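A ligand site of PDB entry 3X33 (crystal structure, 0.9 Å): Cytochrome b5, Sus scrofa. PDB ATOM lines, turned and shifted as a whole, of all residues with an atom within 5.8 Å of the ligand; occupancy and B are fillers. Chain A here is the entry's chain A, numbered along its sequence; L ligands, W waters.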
ATOM      1  N   LEU A  28      -5.731  16.699  23.394  1.00  0.00           N
ATOM      2  CA  LEU A  28      -5.776  15.246  23.600  1.00  0.00           C
ATOM      3  C   LEU A  28      -5.774  14.987  25.098  1.00  0.00           C
ATOM      4  O   LEU A  28      -5.496  15.874  25.897  1.00  0.00           O
ATOM      5  CB  LEU A  28      -4.918  14.452  22.733  1.00  0.00           C
ATOM      6  CG  LEU A  28      -3.453  14.797  22.874  1.00  0.00           C
ATOM      7  CD1 LEU A  28      -2.767  14.386  24.176  1.00  0.00           C
ATOM      8  CD2 LEU A  28      -2.592  14.179  21.716  1.00  0.00           C
ATOM      9  N   LEU A  30      -4.217  12.502  28.170  1.00  0.00           N
ATOM     10  CA  LEU A  30      -3.243  11.541  28.641  1.00  0.00           C
ATOM     11  C   LEU A  30      -3.476  11.347  30.105  1.00  0.00           C
ATOM     12  O   LEU A  30      -3.443  12.322  30.883  1.00  0.00           O
ATOM     13  CB  LEU A  30      -1.803  11.980  28.454  1.00  0.00           C
ATOM     14  CG  LEU A  30      -1.390  12.348  27.024  1.00  0.00           C
ATOM     15  CD1 LEU A  30      -0.034  13.053  27.022  1.00  0.00           C
ATOM     16  CD2 LEU A  30      -1.369  11.158  26.133  1.00  0.00           C
ATOM     17  N   TYR A  35      -4.747  18.170  27.443  1.00  0.00           N
ATOM     18  CA  TYR A  35      -3.606  18.924  26.936  1.00  0.00           C
ATOM     19  C   TYR A  35      -4.013  19.692  25.707  1.00  0.00           C
ATOM     20  O   TYR A  35      -4.599  19.111  24.773  1.00  0.00           O
ATOM     21  CB  TYR A  35      -2.478  17.948  26.568  1.00  0.00           C
ATOM     22  CG  TYR A  35      -1.975  17.146  27.714  1.00  0.00           C
ATOM     23  CD1 TYR A  35      -2.672  16.048  28.213  1.00  0.00           C
ATOM     24  CD2 TYR A  35      -0.825  17.469  28.459  1.00  0.00           C
ATOM     25  CE1 TYR A  35      -2.260  15.338  29.299  1.00  0.00           C
ATOM     26  CE2 TYR A  35      -0.377  16.783  29.505  1.00  0.00           C
ATOM     27  CZ  TYR A  35      -1.107  15.725  29.953  1.00  0.00           C
ATOM     28  OH  TYR A  35      -0.704  14.985  31.050  1.00  0.00           O
ATOM     29  N   LEU A  37      -2.440  21.081  22.644  1.00  0.00           N
ATOM     30  CA  LEU A  37      -1.273  20.939  21.847  1.00  0.00           C
ATOM     31  C   LEU A  37      -1.292  21.767  20.563  1.00  0.00           C
ATOM     32  O   LEU A  37      -0.457  21.558  19.656  1.00  0.00           O
ATOM     33  CB  LEU A  37      -0.984  19.449  21.545  1.00  0.00           C
ATOM     34  CG  LEU A  37      -0.921  18.560  22.759  1.00  0.00           C
ATOM     35  CD1 LEU A  37      -0.498  17.165  22.354  1.00  0.00           C
ATOM     36  CD2 LEU A  37       0.077  19.102  23.800  1.00  0.00           C
ATOM     37  N   PHE A  40       2.040  23.170  20.139  1.00  0.00           N
ATOM     38  CA  PHE A  40       3.070  22.110  20.245  1.00  0.00           C
ATOM     39  C   PHE A  40       3.172  21.241  19.036  1.00  0.00           C
ATOM     40  O   PHE A  40       4.201  20.635  18.847  1.00  0.00           O
ATOM     41  CB  PHE A  40       2.785  21.324  21.559  1.00  0.00           C
ATOM     42  CG  PHE A  40       3.828  20.276  21.811  1.00  0.00           C
ATOM     43  CD1 PHE A  40       5.142  20.681  22.103  1.00  0.00           C
ATOM     44  CD2 PHE A  40       3.587  18.913  21.767  1.00  0.00           C
ATOM     45  CE1 PHE A  40       6.155  19.688  22.343  1.00  0.00           C
ATOM     46  CE2 PHE A  40       4.548  17.958  22.048  1.00  0.00           C
ATOM     47  CZ  PHE A  40       5.861  18.396  22.373  1.00  0.00           C
ATOM     48  N   HIS A  44       6.744  19.228  18.373  1.00  0.00           N
ATOM     49  CA  HIS A  44       6.889  17.919  18.885  1.00  0.00           C
ATOM     50  C   HIS A  44       8.012  17.182  18.166  1.00  0.00           C
ATOM     51  O   HIS A  44       7.947  17.006  16.929  1.00  0.00           O
ATOM     52  CB  HIS A  44       5.526  17.198  18.667  1.00  0.00           C
ATOM     53  CG  HIS A  44       5.531  15.764  19.172  1.00  0.00           C
ATOM     54  ND1 HIS A  44       5.069  14.720  18.388  1.00  0.00           N
ATOM     55  CD2 HIS A  44       5.929  15.209  20.338  1.00  0.00           C
ATOM     56  CE1 HIS A  44       5.109  13.601  19.122  1.00  0.00           C
ATOM     57  NE2 HIS A  44       5.621  13.872  20.310  1.00  0.00           N
ATOM     58  N   PRO A  45       8.980  16.567  18.851  1.00  0.00           N
ATOM     59  CA  PRO A  45      10.045  15.877  18.260  1.00  0.00           C
ATOM     60  C   PRO A  45       9.561  14.685  17.403  1.00  0.00           C
ATOM     61  O   PRO A  45      10.158  14.280  16.429  1.00  0.00           O
ATOM     62  CB  PRO A  45      10.996  15.470  19.352  1.00  0.00           C
ATOM     63  CG  PRO A  45      10.834  16.565  20.352  1.00  0.00           C
ATOM     64  CD  PRO A  45       9.304  16.873  20.351  1.00  0.00           C
ATOM     65  N   GLY A  46       8.436  14.066  17.830  1.00  0.00           N
ATOM     66  CA  GLY A  46       7.904  12.924  17.137  1.00  0.00           C
ATOM     67  C   GLY A  46       7.080  13.354  15.925  1.00  0.00           C
ATOM     68  O   GLY A  46       6.559  12.426  15.282  1.00  0.00           O
ATOM     69  N   VAL A  50       1.621  12.186  14.104  1.00  0.00           N
ATOM     70  CA  VAL A  50       1.196  11.189  15.171  1.00  0.00           C
ATOM     71  C   VAL A  50       0.261  11.846  16.144  1.00  0.00           C
ATOM     72  O   VAL A  50      -0.569  11.189  16.736  1.00  0.00           O
ATOM     73  CB  VAL A  50       2.416  10.639  15.880  1.00  0.00           C
ATOM     74  CG1 VAL A  50       3.117   9.687  15.011  1.00  0.00           C
ATOM     75  CG2 VAL A  50       3.261  11.644  16.637  1.00  0.00           C
ATOM     76  N   LEU A  51       0.414  13.228  16.405  1.00  0.00           N
ATOM     77  CA  LEU A  51      -0.513  13.919  17.229  1.00  0.00           C
ATOM     78  C   LEU A  51      -1.830  14.175  16.559  1.00  0.00           C
ATOM     79  O   LEU A  51      -2.877  13.970  17.138  1.00  0.00           O
ATOM     80  CB  LEU A  51       0.104  15.265  17.699  1.00  0.00           C
ATOM     81  CG  LEU A  51       1.421  15.126  18.455  1.00  0.00           C
ATOM     82  CD1 LEU A  51       1.981  16.447  18.823  1.00  0.00           C
ATOM     83  CD2 LEU A  51       1.315  14.242  19.706  1.00  0.00           C
ATOM     84  N   GLN A  54      -4.380  11.576  16.864  1.00  0.00           N
ATOM     85  CA  GLN A  54      -4.978  11.351  18.153  1.00  0.00           C
ATOM     86  C   GLN A  54      -5.889  12.486  18.617  1.00  0.00           C
ATOM     87  O   GLN A  54      -6.499  12.397  19.691  1.00  0.00           O
ATOM     88  CB  GLN A  54      -3.902  11.185  19.255  1.00  0.00           C
ATOM     89  CG  GLN A  54      -2.907  10.041  18.964  1.00  0.00           C
ATOM     90  CD  GLN A  54      -3.707   8.767  18.695  1.00  0.00           C
ATOM     91  OE1 GLN A  54      -4.575   8.428  19.504  1.00  0.00           O
ATOM     92  NE2 GLN A  54      -3.535   8.039  17.605  1.00  0.00           N
ATOM     93  N   ALA A  59      -5.134   9.546  24.121  1.00  0.00           N
ATOM     94  CA  ALA A  59      -3.935   9.120  23.449  1.00  0.00           C
ATOM     95  C   ALA A  59      -2.984   8.398  24.385  1.00  0.00           C
ATOM     96  O   ALA A  59      -1.832   8.119  24.024  1.00  0.00           O
ATOM     97  CB  ALA A  59      -3.224  10.296  22.770  1.00  0.00           C
ATOM     98  N   ASN A  62      -1.219   5.029  23.186  1.00  0.00           N
ATOM     99  CA  ASN A  62      -0.189   5.271  22.148  1.00  0.00           C
ATOM    100  C   ASN A  62       0.996   6.017  22.705  1.00  0.00           C
ATOM    101  O   ASN A  62       2.138   5.717  22.352  1.00  0.00           O
ATOM    102  CB  ASN A  62      -0.859   6.109  21.035  1.00  0.00           C
ATOM    103  CG  ASN A  62      -1.651   5.210  20.100  1.00  0.00           C
ATOM    104  OD1 ASN A  62      -1.286   4.031  19.996  1.00  0.00           O
ATOM    105  ND2 ASN A  62      -2.646   5.734  19.383  1.00  0.00           N
ATOM    106  N   PHE A  63       0.837   7.099  23.575  1.00  0.00           N
ATOM    107  CA  PHE A  63       1.936   7.828  24.248  1.00  0.00           C
ATOM    108  C   PHE A  63       2.863   6.876  24.975  1.00  0.00           C
ATOM    109  O   PHE A  63       4.089   6.999  24.915  1.00  0.00           O
ATOM    110  CB  PHE A  63       1.284   8.828  25.164  1.00  0.00           C
ATOM    111  CG  PHE A  63       2.274   9.704  25.969  1.00  0.00           C
ATOM    112  CD1 PHE A  63       2.814  10.844  25.455  1.00  0.00           C
ATOM    113  CD2 PHE A  63       2.569   9.337  27.290  1.00  0.00           C
ATOM    114  CE1 PHE A  63       3.672  11.637  26.184  1.00  0.00           C
ATOM    115  CE2 PHE A  63       3.447  10.144  28.020  1.00  0.00           C
ATOM    116  CZ  PHE A  63       3.978  11.276  27.487  1.00  0.00           C
ATOM    117  N   VAL A  66       4.830   4.038  22.545  1.00  0.00           N
ATOM    118  CA  VAL A  66       5.992   4.500  21.842  1.00  0.00           C
ATOM    119  C   VAL A  66       7.156   4.827  22.804  1.00  0.00           C
ATOM    120  O   VAL A  66       8.304   4.859  22.351  1.00  0.00           O
ATOM    121  CB  VAL A  66       5.723   5.752  21.024  1.00  0.00           C
ATOM    122  CG1 VAL A  66       5.370   6.890  21.966  1.00  0.00           C
ATOM    123  CG2 VAL A  66       6.942   6.039  20.135  1.00  0.00           C
ATOM    124  N   GLY A  67       6.842   5.085  24.037  1.00  0.00           N
ATOM    125  CA  GLY A  67       7.839   5.436  25.088  1.00  0.00           C
ATOM    126  C   GLY A  67       8.060   6.942  25.058  1.00  0.00           C
ATOM    127  O   GLY A  67       8.134   7.550  23.955  1.00  0.00           O
ATOM    128  N   HIS A  68       8.206   7.562  26.172  1.00  0.00           N
ATOM    129  CA  HIS A  68       8.509   8.953  26.294  1.00  0.00           C
ATOM    130  C   HIS A  68       9.447   9.144  27.528  1.00  0.00           C
ATOM    131  O   HIS A  68       9.172   8.567  28.606  1.00  0.00           O
ATOM    132  CB  HIS A  68       7.242   9.821  26.489  1.00  0.00           C
ATOM    133  CG  HIS A  68       6.597  10.193  25.177  1.00  0.00           C
ATOM    134  ND1 HIS A  68       5.689   9.433  24.506  1.00  0.00           N
ATOM    135  CD2 HIS A  68       6.782  11.284  24.434  1.00  0.00           C
ATOM    136  CE1 HIS A  68       5.374  10.079  23.371  1.00  0.00           C
ATOM    137  NE2 HIS A  68       6.032  11.220  23.250  1.00  0.00           N
ATOM    138  N   SER A  69      10.429   9.939  27.361  1.00  0.00           N
ATOM    139  CA  SER A  69      11.418  10.223  28.377  1.00  0.00           C
ATOM    140  C   SER A  69      10.782  10.925  29.598  1.00  0.00           C
ATOM    141  O   SER A  69       9.745  11.572  29.486  1.00  0.00           O
ATOM    142  CB  SER A  69      12.555  11.067  27.821  1.00  0.00           C
ATOM    143  OG  SER A  69      12.075  12.398  27.506  1.00  0.00           O
ATOM    144  N   ASP A  71      12.117  13.653  30.526  1.00  0.00           N
ATOM    145  CA  ASP A  71      12.056  15.057  30.057  1.00  0.00           C
ATOM    146  C   ASP A  71      10.778  15.352  29.265  1.00  0.00           C
ATOM    147  O   ASP A  71      10.145  16.429  29.488  1.00  0.00           O
ATOM    148  CB  ASP A  71      13.221  15.272  29.175  1.00  0.00           C
ATOM    149  CG  ASP A  71      14.592  15.423  29.813  1.00  0.00           C
ATOM    150  OD1 ASP A  71      14.652  15.537  31.058  1.00  0.00           O
ATOM    151  OD2 ASP A  71      15.578  15.410  29.046  1.00  0.00           O
ATOM    152  N   ALA A  72      10.369  14.447  28.419  1.00  0.00           N
ATOM    153  CA  ALA A  72       9.121  14.650  27.658  1.00  0.00           C
ATOM    154  C   ALA A  72       7.895  14.723  28.620  1.00  0.00           C
ATOM    155  O   ALA A  72       6.972  15.522  28.363  1.00  0.00           O
ATOM    156  CB  ALA A  72       8.932  13.505  26.664  1.00  0.00           C
ATOM    157  N   ARG A  73       7.891  13.858  29.633  1.00  0.00           N
ATOM    158  CA  ARG A  73       6.759  13.848  30.559  1.00  0.00           C
ATOM    159  C   ARG A  73       6.726  15.131  31.326  1.00  0.00           C
ATOM    160  O   ARG A  73       5.626  15.724  31.576  1.00  0.00           O
ATOM    161  CB  ARG A  73       6.869  12.644  31.442  1.00  0.00           C
ATOM    162  CG  ARG A  73       6.670  11.343  30.619  1.00  0.00           C
ATOM    163  CD  ARG A  73       7.127  10.155  31.403  1.00  0.00           C
ATOM    164  NE  ARG A  73       7.092   8.922  30.539  1.00  0.00           N
ATOM    165  CZ  ARG A  73       6.002   8.190  30.364  1.00  0.00           C
ATOM    166  NH1 ARG A  73       4.847   8.443  31.014  1.00  0.00           N
ATOM    167  NH2 ARG A  73       6.064   7.171  29.477  1.00  0.00           N
ATOM    168  N   LEU A  75       7.847  18.019  30.229  1.00  0.00           N
ATOM    169  CA  LEU A  75       7.420  19.035  29.220  1.00  0.00           C
ATOM    170  C   LEU A  75       5.857  18.971  29.071  1.00  0.00           C
ATOM    171  O   LEU A  75       5.216  20.003  28.874  1.00  0.00           O
ATOM    172  CB  LEU A  75       8.166  18.743  27.948  1.00  0.00           C
ATOM    173  CG  LEU A  75       7.737  19.544  26.762  1.00  0.00           C
ATOM    174  CD1 LEU A  75       7.975  21.157  27.053  1.00  0.00           C
ATOM    175  CD2 LEU A  75       8.465  19.179  25.503  1.00  0.00           C
ATOM    176  N   SER A  76       5.315  17.732  29.072  1.00  0.00           N
ATOM    177  CA  SER A  76       3.870  17.640  28.845  1.00  0.00           C
ATOM    178  C   SER A  76       3.060  18.448  29.847  1.00  0.00           C
ATOM    179  O   SER A  76       1.981  18.917  29.500  1.00  0.00           O
ATOM    180  CB  SER A  76       3.430  16.155  28.862  1.00  0.00           C
ATOM    181  OG  SER A  76       3.407  15.567  30.144  1.00  0.00           O
ATOM    182  N   PHE A  79       1.348  21.861  29.013  1.00  0.00           N
ATOM    183  CA  PHE A  79       0.205  22.015  28.152  1.00  0.00           C
ATOM    184  C   PHE A  79      -1.079  21.622  28.745  1.00  0.00           C
ATOM    185  O   PHE A  79      -2.152  21.639  28.098  1.00  0.00           O
ATOM    186  CB  PHE A  79       0.415  21.154  26.822  1.00  0.00           C
ATOM    187  CG  PHE A  79       1.754  21.458  26.162  1.00  0.00           C
ATOM    188  CD1 PHE A  79       1.959  22.686  25.518  1.00  0.00           C
ATOM    189  CD2 PHE A  79       2.762  20.550  26.190  1.00  0.00           C
ATOM    190  CE1 PHE A  79       3.197  22.962  24.949  1.00  0.00           C
ATOM    191  CE2 PHE A  79       4.007  20.788  25.634  1.00  0.00           C
ATOM    192  CZ  PHE A  79       4.176  21.992  25.032  1.00  0.00           C
HETATM  193  C1  LIG L   1       8.995  11.709  20.737  1.00  0.00           C
HETATM  194  C2  LIG L   1       7.156  15.026  23.747  1.00  0.00           C
HETATM  195  C3  LIG L   1       2.783  13.256  22.947  1.00  0.00           C
HETATM  196  C4  LIG L   1       4.582  10.170  19.733  1.00  0.00           C
HETATM  197  C5  LIG L   1       8.881  12.749  21.710  1.00  0.00           C
HETATM  198  C6  LIG L   1      10.039  13.461  22.304  1.00  0.00           C
HETATM  199  C7  LIG L   1       9.466  14.459  23.088  1.00  0.00           C
HETATM  200  C8  LIG L   1       8.067  14.260  23.019  1.00  0.00           C
HETATM  201  C9  LIG L   1      10.212  15.498  23.898  1.00  0.00           C
HETATM  202  C10 LIG L   1      11.459  13.141  22.057  1.00  0.00           C
HETATM  203  C11 LIG L   1      11.847  11.748  22.725  1.00  0.00           C
HETATM  204  C12 LIG L   1      11.586  11.695  24.175  1.00  0.00           C
HETATM  205  O1  LIG L   1      11.918  12.670  24.924  1.00  0.00           O
HETATM  206  O2  LIG L   1      11.132  10.593  24.664  1.00  0.00           O
HETATM  207  C13 LIG L   1       5.787  14.843  23.799  1.00  0.00           C
HETATM  208  C14 LIG L   1       4.912  15.599  24.657  1.00  0.00           C
HETATM  209  C15 LIG L   1       3.669  15.083  24.410  1.00  0.00           C
HETATM  210  C16 LIG L   1       3.816  14.023  23.458  1.00  0.00           C
HETATM  211  C17 LIG L   1       5.336  16.697  25.492  1.00  0.00           C
HETATM  212  C18 LIG L   1       2.394  15.440  25.080  1.00  0.00           C
HETATM  213  C19 LIG L   1       2.045  16.668  25.490  1.00  0.00           C
HETATM  214  C20 LIG L   1       2.875  12.217  22.050  1.00  0.00           C
HETATM  215  C21 LIG L   1       1.773  11.359  21.590  1.00  0.00           C
HETATM  216  C22 LIG L   1       2.274  10.538  20.706  1.00  0.00           C
HETATM  217  C23 LIG L   1       3.692  10.814  20.558  1.00  0.00           C
HETATM  218  C24 LIG L   1       0.363  11.502  22.180  1.00  0.00           C
HETATM  219  C25 LIG L   1       1.585   9.452  19.888  1.00  0.00           C
HETATM  220  C26 LIG L   1       0.366   9.516  19.562  1.00  0.00           C
HETATM  221  C27 LIG L   1       5.922  10.363  19.694  1.00  0.00           C
HETATM  222  C28 LIG L   1       6.852   9.616  18.830  1.00  0.00           C
HETATM  223  C29 LIG L   1       8.110  10.051  19.173  1.00  0.00           C
HETATM  224  C30 LIG L   1       7.980  11.041  20.195  1.00  0.00           C
HETATM  225  C31 LIG L   1       6.451   8.609  17.847  1.00  0.00           C
HETATM  226  C32 LIG L   1       9.410   9.597  18.613  1.00  0.00           C
HETATM  227  C33 LIG L   1      10.056   8.548  19.541  1.00  0.00           C
HETATM  228  C34 LIG L   1      11.583   8.506  19.323  1.00  0.00           C
HETATM  229  O3  LIG L   1      12.310   9.484  19.583  1.00  0.00           O
HETATM  230  O4  LIG L   1      12.002   7.477  18.829  1.00  0.00           O
HETATM  231  N1  LIG L   1       7.702  13.241  22.167  1.00  0.00           N
HETATM  232  N2  LIG L   1       5.100  13.875  23.095  1.00  0.00           N
HETATM  233  N3  LIG L   1       4.029  11.833  21.425  1.00  0.00           N
HETATM  234  N4  LIG L   1       6.607  11.272  20.502  1.00  0.00           N
HETATM  235 FE1  LIG L   1       5.860  12.552  21.795  1.00  0.00          FE
HETATM  236  O   HOH W   1      12.182  17.257  26.043  1.00  0.00           O
HETATM  237  O   HOH W   2      12.196  12.097  18.664  1.00  0.00           O
HETATM  238  O   HOH W   3      14.496  13.433  24.803  1.00  0.00           O
HETATM  239  O   HOH W   4      12.104  18.348  23.480  1.00  0.00           O
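The side-chain hydroxyl of Ser 69 is in hydrogen-bond range of an oxygen (O1) of the ligand (2.6 Å).
A ring nitrogen (NE2) of His 68 binds an iron atom (FE1) of the ligand, at 2.0 Å.
N of Ser 69 sits at hydrogen-bond distance from O2 of the ligand.
NE2 of His 44 binds FE1 of the ligand, 2.0 Å away.
ND1 of His 68 lies within hydrogen-bond range of O of Phe 63 (2.9 Å).
ND1 of His 44 lies close to N of Gly 46 (3.5 Å).
The side-chain hydroxyl (OG) of Ser 69 sits at hydrogen-bond distance from the backbone NH (N) of Ala 72, at 2.8 Å.
O of His 68 is in hydrogen-bond range of NE of Arg 73, 2.9 Å away.
The side-chain amide nitrogen (NE2) of Gln 54 sits close to the side-chain amide nitrogen (ND2) of Asn 62 (3.0 Å).
The side-chain hydroxyl of Ser 76 sits at hydrogen-bond distance from the backbone carbonyl oxygen of Arg 73 (2.6 Å).
N of Asp 71 sits close to OG of Ser 69 (3.3 Å).
Residues that only touch the ligand: Gln 54, Val 50, Leu 51, Val 66, Phe 63, Ala 72, Gly 46, Phe 40, Leu 37, Pro 45, Ser 76, Ala 59, Asn 62, Leu 30 and Leu 75.
Hydrophobic or aromatic side chains within 4 Å of the ligand: Leu 30, Leu 37, Phe 40, His 44, Pro 45, Val 50, Leu 51, Ala 59, Phe 63, Val 66, His 68, Ala 72 and Leu 75.
Within 4 Å of the ligand: Leu 30, Leu 37, Phe 40, His 44, Pro 45, Gly 46, Val 50, Leu 51, Gln 54, Ala 59, Asn 62, Phe 63, Val 66, His 68, Ser 69, Ala 72, Leu 75 and Ser 76.
The nearest printed residue that does not touch the ligand is Phe 79 (4.01 Å).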
